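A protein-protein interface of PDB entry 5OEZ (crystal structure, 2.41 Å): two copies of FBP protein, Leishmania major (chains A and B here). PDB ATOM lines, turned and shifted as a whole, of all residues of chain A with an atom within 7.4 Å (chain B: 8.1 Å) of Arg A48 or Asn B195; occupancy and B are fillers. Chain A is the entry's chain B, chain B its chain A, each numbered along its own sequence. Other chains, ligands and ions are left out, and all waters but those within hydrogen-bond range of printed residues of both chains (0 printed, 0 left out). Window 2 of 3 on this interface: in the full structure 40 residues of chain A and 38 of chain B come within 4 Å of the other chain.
NH2 of Arg A48 sits at hydrogen-bond distance from OD1 of Asn B195, 2.6 Å away. The guanidinium group of Arg A47 sits close to the guanidinium group of Arg B47.
The backbone carbonyl oxygen (O) of Ser B175 sits at hydrogen-bond distance from the guanidinium group (NH2) of Arg B47, at 3.1 Å. N of Asp B193 is in hydrogen-bond range of O of Glu B198 (2.9 Å). OE2 of Glu A43 lies within salt-bridge range of NH2 of Arg A47 (3.5 Å). The side-chain carboxylate (OD1) of Asp B193 lies within hydrogen-bond range of the backbone NH (N) of Asn B195.
Among the printed residues, merely in contact across the chains: Arg A47 with Ser B175 (3.2 Å), Arg A47 with Pro B194 (3.4 Å), Ile A46 with Ser B175 (3.7 Å) and Met A51 with Asp B193 (3.99 Å).
Arg A48 touches just one residue of chain B: Asn B195. Of the printed residues of chain A, Asn B195 touches Arg A48 (2.6 Å). No residue of chain B comes within 4 Å of Ala A49. Of the printed residues of chain A, Pro B194 touches Arg A47 (3.4 Å). Printed residues of chain A within 4 Å of Asp B193: Met A51 (3.99 Å). Printed residues of chain B within 4 Å of Arg A47: Arg B47 (3.0 Å), Ser B175 (3.2 Å) and Pro B194 (3.4 Å). The nearest residue of chain B that does not touch Arg A48 is Pro B194 (5.4 Å). The nearest printed residue of chain A that does not touch Asn B195 is Arg A47 (6.2 Å).
Hydrophobic or aromatic side chains of chain B within 4 Å of the printed part of chain A: Pro B194. Printed residues of chain A that touch a printed residue of chain B: Ile A46, Arg A47, Arg A48 and Met A51. Among the printed residues, 6 pairs touch across the chains.
Arg B47 touches its own counterpart, Arg A47.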
ATOM      1  N   ILE A  42     -14.625  18.186  11.771  1.00  0.00           N
ATOM      2  CA  ILE A  42     -13.217  18.366  12.124  1.00  0.00           C
ATOM      3  C   ILE A  42     -12.546  17.030  12.490  1.00  0.00           C
ATOM      4  O   ILE A  42     -11.417  16.789  12.103  1.00  0.00           O
ATOM      5  CB  ILE A  42     -13.060  19.395  13.257  1.00  0.00           C
ATOM      6  CG1 ILE A  42     -13.469  20.779  12.752  1.00  0.00           C
ATOM      7  CG2 ILE A  42     -11.621  19.433  13.778  1.00  0.00           C
ATOM      8  CD1 ILE A  42     -13.837  21.756  13.857  1.00  0.00           C
ATOM      9  N   GLU A  43     -13.240  16.202  13.261  1.00  0.00           N
ATOM     10  CA  GLU A  43     -12.762  14.873  13.616  1.00  0.00           C
ATOM     11  C   GLU A  43     -12.467  14.037  12.377  1.00  0.00           C
ATOM     12  O   GLU A  43     -11.422  13.396  12.318  1.00  0.00           O
ATOM     13  CB  GLU A  43     -13.788  14.146  14.484  1.00  0.00           C
ATOM     14  CG  GLU A  43     -13.239  13.024  15.358  1.00  0.00           C
ATOM     15  CD  GLU A  43     -12.987  11.708  14.641  1.00  0.00           C
ATOM     16  OE1 GLU A  43     -13.627  11.420  13.606  1.00  0.00           O
ATOM     17  OE2 GLU A  43     -12.130  10.945  15.143  1.00  0.00           O
ATOM     18  N   LYS A  44     -13.383  14.028  11.409  1.00  0.00           N
ATOM     19  CA  LYS A  44     -13.180  13.280  10.149  1.00  0.00           C
ATOM     20  C   LYS A  44     -11.845  13.672   9.490  1.00  0.00           C
ATOM     21  O   LYS A  44     -11.038  12.807   9.135  1.00  0.00           O
ATOM     22  CB  LYS A  44     -14.350  13.510   9.176  1.00  0.00           C
ATOM     23  CG  LYS A  44     -14.131  13.075   7.719  1.00  0.00           C
ATOM     24  CD  LYS A  44     -14.842  13.998   6.737  1.00  0.00           C
ATOM     25  CE  LYS A  44     -15.065  13.436   5.327  1.00  0.00           C
ATOM     26  NZ  LYS A  44     -16.356  12.716   5.084  1.00  0.00           N
ATOM     27  N   ASN A  45     -11.620  14.973   9.356  1.00  0.00           N
ATOM     28  CA  ASN A  45     -10.392  15.492   8.741  1.00  0.00           C
ATOM     29  C   ASN A  45      -9.127  15.144   9.529  1.00  0.00           C
ATOM     30  O   ASN A  45      -8.121  14.745   8.951  1.00  0.00           O
ATOM     31  CB  ASN A  45     -10.514  16.992   8.521  1.00  0.00           C
ATOM     32  CG  ASN A  45     -11.519  17.318   7.431  1.00  0.00           C
ATOM     33  OD1 ASN A  45     -11.255  17.079   6.263  1.00  0.00           O
ATOM     34  ND2 ASN A  45     -12.679  17.828   7.807  1.00  0.00           N
ATOM     35  N   ILE A  46      -9.205  15.222  10.846  1.00  0.00           N
ATOM     36  CA  ILE A  46      -8.083  14.837  11.682  1.00  0.00           C
ATOM     37  C   ILE A  46      -7.775  13.343  11.546  1.00  0.00           C
ATOM     38  O   ILE A  46      -6.607  12.986  11.425  1.00  0.00           O
ATOM     39  CB  ILE A  46      -8.295  15.242  13.170  1.00  0.00           C
ATOM     40  CG1 ILE A  46      -8.338  16.772  13.312  1.00  0.00           C
ATOM     41  CG2 ILE A  46      -7.166  14.711  14.057  1.00  0.00           C
ATOM     42  CD1 ILE A  46      -8.880  17.258  14.639  1.00  0.00           C
ATOM     43  N   ARG A  47      -8.798  12.475  11.605  1.00  0.00           N
ATOM     44  CA  ARG A  47      -8.602  11.009  11.511  1.00  0.00           C
ATOM     45  C   ARG A  47      -7.788  10.619  10.284  1.00  0.00           C
ATOM     46  O   ARG A  47      -6.936   9.728  10.352  1.00  0.00           O
ATOM     47  CB  ARG A  47      -9.946  10.230  11.521  1.00  0.00           C
ATOM     48  CG  ARG A  47     -10.483   9.914  12.900  1.00  0.00           C
ATOM     49  CD  ARG A  47     -10.097   8.560  13.465  1.00  0.00           C
ATOM     50  NE  ARG A  47     -10.754   7.388  12.887  1.00  0.00           N
ATOM     51  CZ  ARG A  47     -12.012   7.011  13.129  1.00  0.00           C
ATOM     52  NH1 ARG A  47     -12.481   5.906  12.558  1.00  0.00           N
ATOM     53  NH2 ARG A  47     -12.818   7.721  13.923  1.00  0.00           N
ATOM     54  N   ARG A  48      -8.043  11.303   9.170  1.00  0.00           N
ATOM     55  CA  ARG A  48      -7.381  11.012   7.897  1.00  0.00           C
ATOM     56  C   ARG A  48      -6.181  11.911   7.532  1.00  0.00           C
ATOM     57  O   ARG A  48      -5.710  11.870   6.394  1.00  0.00           O
ATOM     58  CB  ARG A  48      -8.424  11.055   6.792  1.00  0.00           C
ATOM     59  CG  ARG A  48      -9.423   9.914   6.871  1.00  0.00           C
ATOM     60  CD  ARG A  48     -10.709  10.385   6.210  1.00  0.00           C
ATOM     61  NE  ARG A  48     -11.564   9.306   5.714  1.00  0.00           N
ATOM     62  CZ  ARG A  48     -12.361   9.396   4.640  1.00  0.00           C
ATOM     63  NH1 ARG A  48     -12.459  10.514   3.909  1.00  0.00           N
ATOM     64  NH2 ARG A  48     -13.070   8.339   4.274  1.00  0.00           N
ATOM     65  N   ALA A  49      -5.674  12.695   8.483  1.00  0.00           N
ATOM     66  CA  ALA A  49      -4.478  13.510   8.261  1.00  0.00           C
ATOM     67  C   ALA A  49      -3.330  12.563   7.873  1.00  0.00           C
ATOM     68  O   ALA A  49      -3.142  11.528   8.514  1.00  0.00           O
ATOM     69  CB  ALA A  49      -4.103  14.272   9.518  1.00  0.00           C
ATOM     70  N   GLY A  50      -2.579  12.909   6.832  1.00  0.00           N
ATOM     71  CA  GLY A  50      -1.433  12.102   6.396  1.00  0.00           C
ATOM     72  C   GLY A  50      -1.678  11.267   5.160  1.00  0.00           C
ATOM     73  O   GLY A  50      -0.783  11.096   4.340  1.00  0.00           O
ATOM     74  N   MET A  51      -2.898  10.769   4.998  1.00  0.00           N
ATOM     75  CA  MET A  51      -3.172   9.745   4.013  1.00  0.00           C
ATOM     76  C   MET A  51      -3.464  10.363   2.671  1.00  0.00           C
ATOM     77  O   MET A  51      -4.396  11.129   2.573  1.00  0.00           O
ATOM     78  CB  MET A  51      -4.374   8.917   4.469  1.00  0.00           C
ATOM     79  CG  MET A  51      -4.327   8.464   5.902  1.00  0.00           C
ATOM     80  SD  MET A  51      -5.153   6.894   6.235  1.00  0.00           S
ATOM     81  CE  MET A  51      -6.785   7.434   6.722  1.00  0.00           C
ATOM     82  N   LEU A  73      -5.694  22.096   8.172  1.00  0.00           N
ATOM     83  CA  LEU A  73      -6.645  21.765   9.238  1.00  0.00           C
ATOM     84  C   LEU A  73      -7.255  22.990   9.921  1.00  0.00           C
ATOM     85  O   LEU A  73      -8.443  22.979  10.244  1.00  0.00           O
ATOM     86  CB  LEU A  73      -5.975  20.861  10.289  1.00  0.00           C
ATOM     87  CG  LEU A  73      -6.145  19.352  10.163  1.00  0.00           C
ATOM     88  CD1 LEU A  73      -7.458  18.954  10.811  1.00  0.00           C
ATOM     89  CD2 LEU A  73      -6.089  18.833   8.731  1.00  0.00           C
ATOM     90  N   ARG B  47     -11.172   3.158  21.320  1.00  0.00           N
ATOM     91  CA  ARG B  47     -12.137   4.124  20.742  1.00  0.00           C
ATOM     92  C   ARG B  47     -13.431   4.226  21.571  1.00  0.00           C
ATOM     93  O   ARG B  47     -13.958   5.322  21.756  1.00  0.00           O
ATOM     94  CB  ARG B  47     -12.483   3.800  19.255  1.00  0.00           C
ATOM     95  CG  ARG B  47     -11.534   4.368  18.228  1.00  0.00           C
ATOM     96  CD  ARG B  47     -11.908   5.693  17.586  1.00  0.00           C
ATOM     97  NE  ARG B  47     -10.803   5.969  16.680  1.00  0.00           N
ATOM     98  CZ  ARG B  47      -9.937   6.992  16.680  1.00  0.00           C
ATOM     99  NH1 ARG B  47     -10.026   8.029  17.509  1.00  0.00           N
ATOM    100  NH2 ARG B  47      -8.966   6.989  15.768  1.00  0.00           N
ATOM    101  N   SER B 175      -5.488  10.235  17.779  1.00  0.00           N
ATOM    102  CA  SER B 175      -6.559  10.619  16.828  1.00  0.00           C
ATOM    103  C   SER B 175      -6.429   9.859  15.518  1.00  0.00           C
ATOM    104  O   SER B 175      -7.428   9.567  14.881  1.00  0.00           O
ATOM    105  CB  SER B 175      -6.610  12.133  16.591  1.00  0.00           C
ATOM    106  OG  SER B 175      -5.314  12.715  16.563  1.00  0.00           O
ATOM    107  N   ALA B 176      -5.198   9.538  15.133  1.00  0.00           N
ATOM    108  CA  ALA B 176      -4.933   8.500  14.153  1.00  0.00           C
ATOM    109  C   ALA B 176      -4.251   7.346  14.868  1.00  0.00           C
ATOM    110  O   ALA B 176      -3.791   7.491  16.003  1.00  0.00           O
ATOM    111  CB  ALA B 176      -4.044   9.026  13.057  1.00  0.00           C
ATOM    112  N   THR B 191      -0.293   4.195   8.653  1.00  0.00           N
ATOM    113  CA  THR B 191      -1.470   4.742   9.304  1.00  0.00           C
ATOM    114  C   THR B 191      -2.681   3.883   8.965  1.00  0.00           C
ATOM    115  O   THR B 191      -2.854   3.466   7.822  1.00  0.00           O
ATOM    116  CB  THR B 191      -1.695   6.204   8.889  1.00  0.00           C
ATOM    117  OG1 THR B 191      -0.531   6.961   9.240  1.00  0.00           O
ATOM    118  CG2 THR B 191      -2.906   6.807   9.607  1.00  0.00           C
ATOM    119  N   LEU B 192      -3.498   3.606   9.977  1.00  0.00           N
ATOM    120  CA  LEU B 192      -4.664   2.761   9.816  1.00  0.00           C
ATOM    121  C   LEU B 192      -5.730   3.530   9.068  1.00  0.00           C
ATOM    122  O   LEU B 192      -6.113   4.607   9.494  1.00  0.00           O
ATOM    123  CB  LEU B 192      -5.198   2.311  11.177  1.00  0.00           C
ATOM    124  CG  LEU B 192      -6.475   1.459  11.217  1.00  0.00           C
ATOM    125  CD1 LEU B 192      -6.308   0.179  10.430  1.00  0.00           C
ATOM    126  CD2 LEU B 192      -6.847   1.146  12.659  1.00  0.00           C
ATOM    127  N   ASP B 193      -6.161   2.992   7.927  1.00  0.00           N
ATOM    128  CA  ASP B 193      -7.311   3.514   7.211  1.00  0.00           C
ATOM    129  C   ASP B 193      -8.539   2.798   7.787  1.00  0.00           C
ATOM    130  O   ASP B 193      -8.766   1.620   7.488  1.00  0.00           O
ATOM    131  CB  ASP B 193      -7.193   3.262   5.710  1.00  0.00           C
ATOM    132  CG  ASP B 193      -8.346   3.875   4.917  1.00  0.00           C
ATOM    133  OD1 ASP B 193      -9.472   4.004   5.456  1.00  0.00           O
ATOM    134  OD2 ASP B 193      -8.140   4.194   3.727  1.00  0.00           O
ATOM    135  N   PRO B 194      -9.324   3.493   8.624  1.00  0.00           N
ATOM    136  CA  PRO B 194     -10.449   2.816   9.270  1.00  0.00           C
ATOM    137  C   PRO B 194     -11.549   2.339   8.293  1.00  0.00           C
ATOM    138  O   PRO B 194     -12.281   1.402   8.608  1.00  0.00           O
ATOM    139  CB  PRO B 194     -10.983   3.874  10.231  1.00  0.00           C
ATOM    140  CG  PRO B 194     -10.608   5.173   9.608  1.00  0.00           C
ATOM    141  CD  PRO B 194      -9.317   4.943   8.894  1.00  0.00           C
ATOM    142  N   ASN B 195     -11.633   2.953   7.117  1.00  0.00           N
ATOM    143  CA  ASN B 195     -12.576   2.533   6.085  1.00  0.00           C
ATOM    144  C   ASN B 195     -12.293   1.180   5.428  1.00  0.00           C
ATOM    145  O   ASN B 195     -13.227   0.558   4.934  1.00  0.00           O
ATOM    146  CB  ASN B 195     -12.692   3.619   5.008  1.00  0.00           C
ATOM    147  CG  ASN B 195     -13.213   4.941   5.556  1.00  0.00           C
ATOM    148  OD1 ASN B 195     -12.705   5.986   5.190  1.00  0.00           O
ATOM    149  ND2 ASN B 195     -14.200   4.900   6.440  1.00  0.00           N
ATOM    150  N   ILE B 196     -11.043   0.730   5.410  1.00  0.00           N
ATOM    151  CA  ILE B 196     -10.711  -0.601   4.863  1.00  0.00           C
ATOM    152  C   ILE B 196     -10.009  -1.538   5.848  1.00  0.00           C
ATOM    153  O   ILE B 196      -9.694  -2.662   5.492  1.00  0.00           O
ATOM    154  CB  ILE B 196      -9.903  -0.487   3.552  1.00  0.00           C
ATOM    155  CG1 ILE B 196      -8.584   0.276   3.759  1.00  0.00           C
ATOM    156  CG2 ILE B 196     -10.750   0.194   2.492  1.00  0.00           C
ATOM    157  CD1 ILE B 196      -7.749   0.454   2.510  1.00  0.00           C
ATOM    158  N   GLY B 197      -9.791  -1.092   7.084  1.00  0.00           N
ATOM    159  CA  GLY B 197      -9.083  -1.873   8.092  1.00  0.00           C
ATOM    160  C   GLY B 197      -7.721  -2.374   7.651  1.00  0.00           C
ATOM    161  O   GLY B 197      -7.411  -3.556   7.808  1.00  0.00           O
ATOM    162  N   GLU B 198      -6.933  -1.490   7.057  1.00  0.00           N
ATOM    163  CA  GLU B 198      -5.592  -1.834   6.619  1.00  0.00           C
ATOM    164  C   GLU B 198      -4.678  -0.695   7.001  1.00  0.00           C
ATOM    165  O   GLU B 198      -5.086   0.473   7.017  1.00  0.00           O
ATOM    166  CB  GLU B 198      -5.525  -2.032   5.099  1.00  0.00           C
ATOM    167  CG  GLU B 198      -6.339  -3.192   4.545  1.00  0.00           C
ATOM    168  CD  GLU B 198      -5.700  -4.569   4.726  1.00  0.00           C
ATOM    169  OE1 GLU B 198      -4.505  -4.670   5.043  1.00  0.00           O
ATOM    170  OE2 GLU B 198      -6.405  -5.582   4.515  1.00  0.00           O
ATOM    171  N   THR B 202       2.464   5.785   4.975  1.00  0.00           N
ATOM    172  CA  THR B 202       2.342   7.241   5.007  1.00  0.00           C
ATOM    173  C   THR B 202       3.654   8.019   5.289  1.00  0.00           C
ATOM    174  O   THR B 202       3.761   9.175   4.885  1.00  0.00           O
ATOM    175  CB  THR B 202       1.269   7.672   6.044  1.00  0.00           C
ATOM    176  OG1 THR B 202       1.517   7.032   7.304  1.00  0.00           O
ATOM    177  CG2 THR B 202      -0.132   7.291   5.556  1.00  0.00           C
